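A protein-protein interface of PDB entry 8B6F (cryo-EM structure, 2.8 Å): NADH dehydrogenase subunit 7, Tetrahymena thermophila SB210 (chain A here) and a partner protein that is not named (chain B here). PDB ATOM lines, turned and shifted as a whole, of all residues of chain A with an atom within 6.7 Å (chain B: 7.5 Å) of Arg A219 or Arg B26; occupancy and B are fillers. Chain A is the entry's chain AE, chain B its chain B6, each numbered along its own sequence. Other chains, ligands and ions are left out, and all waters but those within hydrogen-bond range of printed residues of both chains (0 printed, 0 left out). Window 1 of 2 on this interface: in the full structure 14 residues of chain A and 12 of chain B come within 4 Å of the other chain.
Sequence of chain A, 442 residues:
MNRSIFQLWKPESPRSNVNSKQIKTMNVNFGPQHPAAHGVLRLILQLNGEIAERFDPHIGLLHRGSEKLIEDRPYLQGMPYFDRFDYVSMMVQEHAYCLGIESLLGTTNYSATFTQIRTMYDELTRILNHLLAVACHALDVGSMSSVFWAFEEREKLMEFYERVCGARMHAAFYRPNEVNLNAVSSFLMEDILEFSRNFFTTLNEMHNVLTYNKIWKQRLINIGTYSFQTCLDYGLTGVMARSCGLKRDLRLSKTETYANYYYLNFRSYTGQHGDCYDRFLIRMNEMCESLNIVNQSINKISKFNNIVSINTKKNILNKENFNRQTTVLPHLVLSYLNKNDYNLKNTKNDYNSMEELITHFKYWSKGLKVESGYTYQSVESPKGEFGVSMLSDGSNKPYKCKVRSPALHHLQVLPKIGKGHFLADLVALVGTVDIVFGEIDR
The backbone carbonyl oxygen (O) of Val A141 lies within hydrogen-bond range of the backbone NH (N) of Arg B26, at 3.3 Å. The backbone carbonyl oxygen of Thr B23 sits at hydrogen-bond distance from the side-chain hydroxyl of Ser A143 (3.5 Å). OH of Tyr B27 is in hydrogen-bond range of OE1 of Gln A218 (2.8 Å). O of Gln A218 sits at hydrogen-bond distance from NE2 of Gln B31 (2.9 Å). The guanidinium group (NH1) of Arg A219 is in hydrogen-bond range of the backbone carbonyl oxygen (O) of Arg B26 (3.3 Å). OD2 of Asp A425 is in salt-bridge range of NH1 of Arg B28 (3.0 Å).
The backbone carbonyl oxygen (O) of Ala A424 is in hydrogen-bond range of the guanidinium group (NH2) of Arg A219, at 3.1 Å. The guanidinium group (NE) of Arg B28 is in salt-bridge range of the side-chain carboxylate (OD1) of Asp B30. The guanidinium group of Arg B28 lies close to the side-chain amide nitrogen of Gln B31, at 2.9 Å.
Arg A219 touches just these residues of chain B: Arg B26 (3.3 Å), Tyr B27 (3.6 Å), Arg B28 (3.2 Å) and Gln B31 (3.96 Å). Of the printed residues of chain A, Arg B26 touches Asp A140, Val A141, Gly A142 and Arg A219. Printed residues of chain B within 4 Å of Asp A425: Arg B28 (2.3 Å). Of the printed residues of chain A, Pro B25 touches Val A141, Ser A143 and Ile A215. Of the printed residues of chain A, Thr B23 touches Ser A143 (3.5 Å). Printed residues of chain B within 4 Å of Ala A424: Arg B28. Of the printed residues of chain A, Leu B24 touches Gly A142 (3.999 Å) and Ser A143 (3.97 Å). The nearest printed residue of chain A that does not touch Leu B24 is Ile A215 (4.5 Å).
Of the 9 printed residues of chain B, 7 touch a printed residue of chain A. Among the printed residues, Asp or Glu carboxylates within 4 Å of a Lys or Arg side-chain nitrogen of the other chain: Asp A425 with Arg B28 (2.3 Å).
Among the printed residues, merely in contact across the chains: Asp A140 with Arg B26, Val A141 with Pro B25, Gly A142 with Leu B24, Gly A142 with Arg B26, Ser A143 with Leu B24, Ser A143 with Pro B25, Ile A215 with Pro B25, Ile A215 with Tyr B27, Arg A219 with Tyr B27, Arg A219 with Arg B28, Arg A219 with Gln B31 and Ala A424 with Arg B28.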
ATOM      1  N   LEU A 139     -15.801  -8.652  29.155  1.00  0.00           N
ATOM      2  CA  LEU A 139     -14.535  -8.862  28.463  1.00  0.00           C
ATOM      3  C   LEU A 139     -14.366 -10.319  28.057  1.00  0.00           C
ATOM      4  O   LEU A 139     -13.924 -10.614  26.941  1.00  0.00           O
ATOM      5  CB  LEU A 139     -13.374  -8.413  29.350  1.00  0.00           C
ATOM      6  CG  LEU A 139     -11.993  -8.372  28.691  1.00  0.00           C
ATOM      7  CD1 LEU A 139     -11.950  -7.339  27.575  1.00  0.00           C
ATOM      8  CD2 LEU A 139     -10.920  -8.082  29.723  1.00  0.00           C
ATOM      9  N   ASP A 140     -14.711 -11.247  28.950  1.00  0.00           N
ATOM     10  CA  ASP A 140     -14.625 -12.663  28.612  1.00  0.00           C
ATOM     11  C   ASP A 140     -15.568 -13.017  27.471  1.00  0.00           C
ATOM     12  O   ASP A 140     -15.196 -13.764  26.557  1.00  0.00           O
ATOM     13  CB  ASP A 140     -14.941 -13.513  29.841  1.00  0.00           C
ATOM     14  CG  ASP A 140     -13.941 -13.310  30.960  1.00  0.00           C
ATOM     15  OD1 ASP A 140     -12.948 -12.586  30.747  1.00  0.00           O
ATOM     16  OD2 ASP A 140     -14.151 -13.876  32.054  1.00  0.00           O
ATOM     17  N   VAL A 141     -16.796 -12.497  27.504  1.00  0.00           N
ATOM     18  CA  VAL A 141     -17.750 -12.807  26.447  1.00  0.00           C
ATOM     19  C   VAL A 141     -17.304 -12.202  25.122  1.00  0.00           C
ATOM     20  O   VAL A 141     -17.580 -12.762  24.055  1.00  0.00           O
ATOM     21  CB  VAL A 141     -19.159 -12.332  26.848  1.00  0.00           C
ATOM     22  CG1 VAL A 141     -20.137 -12.489  25.692  1.00  0.00           C
ATOM     23  CG2 VAL A 141     -19.649 -13.109  28.057  1.00  0.00           C
ATOM     24  N   GLY A 142     -16.619 -11.062  25.157  1.00  0.00           N
ATOM     25  CA  GLY A 142     -16.099 -10.468  23.941  1.00  0.00           C
ATOM     26  C   GLY A 142     -16.168  -8.956  23.896  1.00  0.00           C
ATOM     27  O   GLY A 142     -15.357  -8.321  23.217  1.00  0.00           O
ATOM     28  N   SER A 143     -17.118  -8.363  24.613  1.00  0.00           N
ATOM     29  CA  SER A 143     -17.245  -6.913  24.607  1.00  0.00           C
ATOM     30  C   SER A 143     -16.032  -6.279  25.276  1.00  0.00           C
ATOM     31  O   SER A 143     -15.591  -6.713  26.341  1.00  0.00           O
ATOM     32  CB  SER A 143     -18.529  -6.493  25.323  1.00  0.00           C
ATOM     33  OG  SER A 143     -18.708  -5.088  25.273  1.00  0.00           O
ATOM     34  N   LYS A 214     -28.816  -8.950  21.222  1.00  0.00           N
ATOM     35  CA  LYS A 214     -29.191 -10.322  20.896  1.00  0.00           C
ATOM     36  C   LYS A 214     -28.052 -11.288  21.190  1.00  0.00           C
ATOM     37  O   LYS A 214     -28.278 -12.383  21.716  1.00  0.00           O
ATOM     38  CB  LYS A 214     -29.600 -10.405  19.426  1.00  0.00           C
ATOM     39  CG  LYS A 214     -30.025 -11.784  18.957  1.00  0.00           C
ATOM     40  CD  LYS A 214     -30.342 -11.767  17.471  1.00  0.00           C
ATOM     41  CE  LYS A 214     -30.576 -13.166  16.936  1.00  0.00           C
ATOM     42  NZ  LYS A 214     -30.899 -13.155  15.482  1.00  0.00           N
ATOM     43  N   ILE A 215     -26.820 -10.903  20.854  1.00  0.00           N
ATOM     44  CA  ILE A 215     -25.677 -11.778  21.097  1.00  0.00           C
ATOM     45  C   ILE A 215     -25.484 -11.990  22.591  1.00  0.00           C
ATOM     46  O   ILE A 215     -25.233 -13.111  23.046  1.00  0.00           O
ATOM     47  CB  ILE A 215     -24.413 -11.195  20.436  1.00  0.00           C
ATOM     48  CG1 ILE A 215     -24.626 -11.046  18.929  1.00  0.00           C
ATOM     49  CG2 ILE A 215     -23.210 -12.088  20.705  1.00  0.00           C
ATOM     50  CD1 ILE A 215     -23.559 -10.236  18.243  1.00  0.00           C
ATOM     51  N   TRP A 216     -25.599 -10.920  23.379  1.00  0.00           N
ATOM     52  CA  TRP A 216     -25.458 -11.049  24.825  1.00  0.00           C
ATOM     53  C   TRP A 216     -26.546 -11.947  25.400  1.00  0.00           C
ATOM     54  O   TRP A 216     -26.276 -12.787  26.267  1.00  0.00           O
ATOM     55  CB  TRP A 216     -25.493  -9.663  25.472  1.00  0.00           C
ATOM     56  CG  TRP A 216     -25.171  -9.655  26.935  1.00  0.00           C
ATOM     57  CD1 TRP A 216     -26.054  -9.541  27.966  1.00  0.00           C
ATOM     58  CD2 TRP A 216     -23.871  -9.750  27.527  1.00  0.00           C
ATOM     59  NE1 TRP A 216     -25.385  -9.564  29.165  1.00  0.00           N
ATOM     60  CE2 TRP A 216     -24.044  -9.691  28.922  1.00  0.00           C
ATOM     61  CE3 TRP A 216     -22.579  -9.883  27.012  1.00  0.00           C
ATOM     62  CZ2 TRP A 216     -22.972  -9.759  29.809  1.00  0.00           C
ATOM     63  CZ3 TRP A 216     -21.517  -9.951  27.894  1.00  0.00           C
ATOM     64  CH2 TRP A 216     -21.720  -9.890  29.278  1.00  0.00           C
ATOM     65  N   LYS A 217     -27.787 -11.780  24.937  1.00  0.00           N
ATOM     66  CA  LYS A 217     -28.877 -12.623  25.419  1.00  0.00           C
ATOM     67  C   LYS A 217     -28.653 -14.084  25.051  1.00  0.00           C
ATOM     68  O   LYS A 217     -28.915 -14.982  25.860  1.00  0.00           O
ATOM     69  CB  LYS A 217     -30.212 -12.123  24.870  1.00  0.00           C
ATOM     70  CG  LYS A 217     -30.717 -10.868  25.557  1.00  0.00           C
ATOM     71  CD  LYS A 217     -32.175 -10.593  25.230  1.00  0.00           C
ATOM     72  CE  LYS A 217     -32.365 -10.245  23.770  1.00  0.00           C
ATOM     73  NZ  LYS A 217     -33.782  -9.898  23.471  1.00  0.00           N
ATOM     74  N   GLN A 218     -28.176 -14.346  23.834  1.00  0.00           N
ATOM     75  CA  GLN A 218     -27.935 -15.723  23.416  1.00  0.00           C
ATOM     76  C   GLN A 218     -26.724 -16.318  24.120  1.00  0.00           C
ATOM     77  O   GLN A 218     -26.637 -17.541  24.270  1.00  0.00           O
ATOM     78  CB  GLN A 218     -27.763 -15.794  21.899  1.00  0.00           C
ATOM     79  CG  GLN A 218     -29.038 -15.478  21.136  1.00  0.00           C
ATOM     80  CD  GLN A 218     -28.863 -15.583  19.639  1.00  0.00           C
ATOM     81  OE1 GLN A 218     -27.749 -15.728  19.139  1.00  0.00           O
ATOM     82  NE2 GLN A 218     -29.970 -15.514  18.911  1.00  0.00           N
ATOM     83  N   ARG A 219     -25.786 -15.479  24.554  1.00  0.00           N
ATOM     84  CA  ARG A 219     -24.621 -15.973  25.278  1.00  0.00           C
ATOM     85  C   ARG A 219     -24.958 -16.336  26.721  1.00  0.00           C
ATOM     86  O   ARG A 219     -24.451 -17.336  27.239  1.00  0.00           O
ATOM     87  CB  ARG A 219     -23.502 -14.934  25.243  1.00  0.00           C
ATOM     88  CG  ARG A 219     -22.856 -14.754  23.875  1.00  0.00           C
ATOM     89  CD  ARG A 219     -21.841 -15.847  23.560  1.00  0.00           C
ATOM     90  NE  ARG A 219     -20.750 -15.884  24.528  1.00  0.00           N
ATOM     91  CZ  ARG A 219     -19.567 -16.438  24.307  1.00  0.00           C
ATOM     92  NH1 ARG A 219     -19.266 -16.988  23.144  1.00  0.00           N
ATOM     93  NH2 ARG A 219     -18.658 -16.436  25.278  1.00  0.00           N
ATOM     94  N   LEU A 220     -25.803 -15.550  27.392  1.00  0.00           N
ATOM     95  CA  LEU A 220     -26.053 -15.752  28.816  1.00  0.00           C
ATOM     96  C   LEU A 220     -27.333 -16.536  29.095  1.00  0.00           C
ATOM     97  O   LEU A 220     -27.318 -17.448  29.924  1.00  0.00           O
ATOM     98  CB  LEU A 220     -26.110 -14.397  29.532  1.00  0.00           C
ATOM     99  CG  LEU A 220     -24.841 -13.539  29.519  1.00  0.00           C
ATOM    100  CD1 LEU A 220     -24.898 -12.531  30.646  1.00  0.00           C
ATOM    101  CD2 LEU A 220     -23.568 -14.361  29.609  1.00  0.00           C
ATOM    102  N   ILE A 221     -28.446 -16.190  28.445  1.00  0.00           N
ATOM    103  CA  ILE A 221     -29.722 -16.808  28.791  1.00  0.00           C
ATOM    104  C   ILE A 221     -29.602 -18.321  28.705  1.00  0.00           C
ATOM    105  O   ILE A 221     -29.048 -18.867  27.746  1.00  0.00           O
ATOM    106  CB  ILE A 221     -30.873 -16.296  27.907  1.00  0.00           C
ATOM    107  CG1 ILE A 221     -31.160 -14.826  28.202  1.00  0.00           C
ATOM    108  CG2 ILE A 221     -32.137 -17.124  28.123  1.00  0.00           C
ATOM    109  CD1 ILE A 221     -31.961 -14.161  27.132  1.00  0.00           C
ATOM    110  N   ASN A 222     -30.137 -19.003  29.714  1.00  0.00           N
ATOM    111  CA  ASN A 222     -30.192 -20.462  29.740  1.00  0.00           C
ATOM    112  C   ASN A 222     -28.809 -21.102  29.759  1.00  0.00           C
ATOM    113  O   ASN A 222     -28.629 -22.226  29.288  1.00  0.00           O
ATOM    114  CB  ASN A 222     -31.000 -21.011  28.565  1.00  0.00           C
ATOM    115  CG  ASN A 222     -31.863 -22.189  28.962  1.00  0.00           C
ATOM    116  OD1 ASN A 222     -31.353 -23.261  29.288  1.00  0.00           O
ATOM    117  ND2 ASN A 222     -33.174 -21.995  28.951  1.00  0.00           N
ATOM    118  N   ILE A 223     -27.827 -20.402  30.313  1.00  0.00           N
ATOM    119  CA  ILE A 223     -26.494 -20.947  30.517  1.00  0.00           C
ATOM    120  C   ILE A 223     -26.285 -20.931  32.020  1.00  0.00           C
ATOM    121  O   ILE A 223     -26.536 -19.913  32.675  1.00  0.00           O
ATOM    122  CB  ILE A 223     -25.410 -20.144  29.768  1.00  0.00           C
ATOM    123  CG1 ILE A 223     -25.305 -20.597  28.310  1.00  0.00           C
ATOM    124  CG2 ILE A 223     -24.049 -20.289  30.423  1.00  0.00           C
ATOM    125  CD1 ILE A 223     -26.365 -20.046  27.407  1.00  0.00           C
ATOM    126  N   CYS A 276     -27.109 -17.078  33.825  1.00  0.00           N
ATOM    127  CA  CYS A 276     -26.139 -15.986  33.801  1.00  0.00           C
ATOM    128  C   CYS A 276     -26.804 -14.656  33.480  1.00  0.00           C
ATOM    129  O   CYS A 276     -26.400 -13.609  34.000  1.00  0.00           O
ATOM    130  CB  CYS A 276     -25.041 -16.284  32.782  1.00  0.00           C
ATOM    131  SG  CYS A 276     -24.006 -17.700  33.188  1.00  0.00           S
ATOM    132  N   LEU A 423     -16.537 -24.565  25.709  1.00  0.00           N
ATOM    133  CA  LEU A 423     -15.466 -23.768  26.296  1.00  0.00           C
ATOM    134  C   LEU A 423     -15.837 -22.291  26.332  1.00  0.00           C
ATOM    135  O   LEU A 423     -15.536 -21.591  27.305  1.00  0.00           O
ATOM    136  CB  LEU A 423     -14.171 -23.979  25.512  1.00  0.00           C
ATOM    137  CG  LEU A 423     -12.915 -23.304  26.066  1.00  0.00           C
ATOM    138  CD1 LEU A 423     -12.557 -23.858  27.437  1.00  0.00           C
ATOM    139  CD2 LEU A 423     -11.759 -23.475  25.098  1.00  0.00           C
ATOM    140  N   ALA A 424     -16.490 -21.797  25.278  1.00  0.00           N
ATOM    141  CA  ALA A 424     -16.925 -20.406  25.257  1.00  0.00           C
ATOM    142  C   ALA A 424     -17.973 -20.131  26.326  1.00  0.00           C
ATOM    143  O   ALA A 424     -18.068 -19.006  26.828  1.00  0.00           O
ATOM    144  CB  ALA A 424     -17.463 -20.046  23.875  1.00  0.00           C
ATOM    145  N   ASP A 425     -18.783 -21.131  26.666  1.00  0.00           N
ATOM    146  CA  ASP A 425     -19.723 -20.994  27.771  1.00  0.00           C
ATOM    147  C   ASP A 425     -19.038 -21.120  29.123  1.00  0.00           C
ATOM    148  O   ASP A 425     -19.460 -20.472  30.087  1.00  0.00           O
ATOM    149  CB  ASP A 425     -20.825 -22.044  27.656  1.00  0.00           C
ATOM    150  CG  ASP A 425     -21.790 -21.757  26.529  1.00  0.00           C
ATOM    151  OD1 ASP A 425     -21.978 -20.569  26.195  1.00  0.00           O
ATOM    152  OD2 ASP A 425     -22.364 -22.718  25.977  1.00  0.00           O
ATOM    153  N   VAL A 427     -15.967 -20.096  29.845  1.00  0.00           N
ATOM    154  CA  VAL A 427     -15.299 -18.828  30.125  1.00  0.00           C
ATOM    155  C   VAL A 427     -16.310 -17.789  30.586  1.00  0.00           C
ATOM    156  O   VAL A 427     -15.957 -16.845  31.301  1.00  0.00           O
ATOM    157  CB  VAL A 427     -14.501 -18.339  28.905  1.00  0.00           C
ATOM    158  CG1 VAL A 427     -13.408 -19.334  28.568  1.00  0.00           C
ATOM    159  CG2 VAL A 427     -15.410 -18.113  27.716  1.00  0.00           C
ATOM    160  N   ALA A 428     -17.569 -17.927  30.177  1.00  0.00           N
ATOM    161  CA  ALA A 428     -18.610 -17.052  30.699  1.00  0.00           C
ATOM    162  C   ALA A 428     -19.016 -17.466  32.108  1.00  0.00           C
ATOM    163  O   ALA A 428     -19.296 -16.610  32.953  1.00  0.00           O
ATOM    164  CB  ALA A 428     -19.824 -17.063  29.770  1.00  0.00           C
ATOM    165  N   THR B  23     -17.551  -2.658  19.919  1.00  0.00           N
ATOM    166  CA  THR B  23     -18.868  -2.645  20.553  1.00  0.00           C
ATOM    167  C   THR B  23     -19.379  -4.051  20.865  1.00  0.00           C
ATOM    168  O   THR B  23     -19.648  -4.376  22.025  1.00  0.00           O
ATOM    169  CB  THR B  23     -19.892  -1.925  19.661  1.00  0.00           C
ATOM    170  OG1 THR B  23     -20.079  -2.658  18.444  1.00  0.00           O
ATOM    171  CG2 THR B  23     -19.461  -0.508  19.352  1.00  0.00           C
ATOM    172  N   LEU B  24     -19.521  -4.887  19.842  1.00  0.00           N
ATOM    173  CA  LEU B  24     -20.309  -6.103  19.965  1.00  0.00           C
ATOM    174  C   LEU B  24     -19.570  -7.203  20.723  1.00  0.00           C
ATOM    175  O   LEU B  24     -18.338  -7.205  20.797  1.00  0.00           O
ATOM    176  CB  LEU B  24     -20.702  -6.616  18.585  1.00  0.00           C
ATOM    177  CG  LEU B  24     -21.759  -5.808  17.831  1.00  0.00           C
ATOM    178  CD1 LEU B  24     -21.999  -6.415  16.467  1.00  0.00           C
ATOM    179  CD2 LEU B  24     -23.066  -5.726  18.604  1.00  0.00           C
ATOM    180  N   PRO B  25     -20.312  -8.160  21.303  1.00  0.00           N
ATOM    181  CA  PRO B  25     -19.673  -9.346  21.893  1.00  0.00           C
ATOM    182  C   PRO B  25     -19.227 -10.335  20.831  1.00  0.00           C
ATOM    183  O   PRO B  25     -19.274 -10.028  19.638  1.00  0.00           O
ATOM    184  CB  PRO B  25     -20.774  -9.944  22.784  1.00  0.00           C
ATOM    185  CG  PRO B  25     -21.877  -8.937  22.815  1.00  0.00           C
ATOM    186  CD  PRO B  25     -21.761  -8.149  21.558  1.00  0.00           C
ATOM    187  N   ARG B  26     -18.778 -11.516  21.251  1.00  0.00           N
ATOM    188  CA  ARG B  26     -18.344 -12.567  20.343  1.00  0.00           C
ATOM    189  C   ARG B  26     -19.304 -13.749  20.412  1.00  0.00           C
ATOM    190  O   ARG B  26     -19.757 -14.131  21.495  1.00  0.00           O
ATOM    191  CB  ARG B  26     -16.920 -13.023  20.673  1.00  0.00           C
ATOM    192  CG  ARG B  26     -16.437 -14.187  19.830  1.00  0.00           C
ATOM    193  CD  ARG B  26     -14.936 -14.395  19.956  1.00  0.00           C
ATOM    194  NE  ARG B  26     -14.492 -14.450  21.344  1.00  0.00           N
ATOM    195  CZ  ARG B  26     -13.947 -13.437  22.008  1.00  0.00           C
ATOM    196  NH1 ARG B  26     -13.761 -12.255  21.441  1.00  0.00           N
ATOM    197  NH2 ARG B  26     -13.580 -13.615  23.272  1.00  0.00           N
ATOM    198  N   TYR B  27     -19.612 -14.318  19.249  1.00  0.00           N
ATOM    199  CA  TYR B  27     -20.510 -15.458  19.146  1.00  0.00           C
ATOM    200  C   TYR B  27     -19.784 -16.754  19.504  1.00  0.00           C
ATOM    201  O   TYR B  27     -18.559 -16.803  19.633  1.00  0.00           O
ATOM    202  CB  TYR B  27     -21.073 -15.571  17.727  1.00  0.00           C
ATOM    203  CG  TYR B  27     -22.531 -15.201  17.585  1.00  0.00           C
ATOM    204  CD1 TYR B  27     -23.513 -15.869  18.305  1.00  0.00           C
ATOM    205  CD2 TYR B  27     -22.928 -14.211  16.699  1.00  0.00           C
ATOM    206  CE1 TYR B  27     -24.846 -15.539  18.164  1.00  0.00           C
ATOM    207  CE2 TYR B  27     -24.256 -13.874  16.552  1.00  0.00           C
ATOM    208  CZ  TYR B  27     -25.210 -14.541  17.287  1.00  0.00           C
ATOM    209  OH  TYR B  27     -26.537 -14.210  17.141  1.00  0.00           O
ATOM    210  N   ARG B  28     -20.565 -17.819  19.663  1.00  0.00           N
ATOM    211  CA  ARG B  28     -20.046 -19.178  19.696  1.00  0.00           C
ATOM    212  C   ARG B  28     -20.150 -19.787  18.304  1.00  0.00           C
ATOM    213  O   ARG B  28     -21.079 -19.491  17.549  1.00  0.00           O
ATOM    214  CB  ARG B  28     -20.807 -20.049  20.696  1.00  0.00           C
ATOM    215  CG  ARG B  28     -20.636 -19.654  22.148  1.00  0.00           C
ATOM    216  CD  ARG B  28     -20.828 -20.854  23.065  1.00  0.00           C
ATOM    217  NE  ARG B  28     -22.054 -21.593  22.782  1.00  0.00           N
ATOM    218  CZ  ARG B  28     -23.216 -21.401  23.390  1.00  0.00           C
ATOM    219  NH1 ARG B  28     -23.367 -20.472  24.319  1.00  0.00           N
ATOM    220  NH2 ARG B  28     -24.254 -22.162  23.060  1.00  0.00           N
ATOM    221  N   PHE B  29     -19.185 -20.644  17.965  1.00  0.00           N
ATOM    222  CA  PHE B  29     -19.185 -21.234  16.630  1.00  0.00           C
ATOM    223  C   PHE B  29     -20.429 -22.084  16.406  1.00  0.00           C
ATOM    224  O   PHE B  29     -21.040 -22.029  15.332  1.00  0.00           O
ATOM    225  CB  PHE B  29     -17.909 -22.053  16.400  1.00  0.00           C
ATOM    226  CG  PHE B  29     -17.630 -23.078  17.461  1.00  0.00           C
ATOM    227  CD1 PHE B  29     -18.172 -24.349  17.377  1.00  0.00           C
ATOM    228  CD2 PHE B  29     -16.788 -22.782  18.519  1.00  0.00           C
ATOM    229  CE1 PHE B  29     -17.903 -25.295  18.344  1.00  0.00           C
ATOM    230  CE2 PHE B  29     -16.516 -23.724  19.488  1.00  0.00           C
ATOM    231  CZ  PHE B  29     -17.074 -24.982  19.400  1.00  0.00           C
ATOM    232  N   ASP B  30     -20.816 -22.888  17.399  1.00  0.00           N
ATOM    233  CA  ASP B  30     -22.016 -23.704  17.252  1.00  0.00           C
ATOM    234  C   ASP B  30     -23.263 -22.835  17.137  1.00  0.00           C
ATOM    235  O   ASP B  30     -24.144 -23.106  16.315  1.00  0.00           O
ATOM    236  CB  ASP B  30     -22.147 -24.669  18.426  1.00  0.00           C
ATOM    237  CG  ASP B  30     -22.310 -23.954  19.745  1.00  0.00           C
ATOM    238  OD1 ASP B  30     -21.610 -22.944  19.959  1.00  0.00           O
ATOM    239  OD2 ASP B  30     -23.145 -24.389  20.565  1.00  0.00           O
ATOM    240  N   GLN B  31     -23.360 -21.790  17.962  1.00  0.00           N
ATOM    241  CA  GLN B  31     -24.518 -20.903  17.899  1.00  0.00           C
ATOM    242  C   GLN B  31     -24.648 -20.265  16.524  1.00  0.00           C
ATOM    243  O   GLN B  31     -25.728 -20.270  15.924  1.00  0.00           O
ATOM    244  CB  GLN B  31     -24.412 -19.823  18.974  1.00  0.00           C
ATOM    245  CG  GLN B  31     -24.694 -20.316  20.375  1.00  0.00           C
ATOM    246  CD  GLN B  31     -24.641 -19.199  21.391  1.00  0.00           C
ATOM    247  OE1 GLN B  31     -23.983 -18.182  21.177  1.00  0.00           O
ATOM    248  NE2 GLN B  31     -25.345 -19.377  22.501  1.00  0.00           N
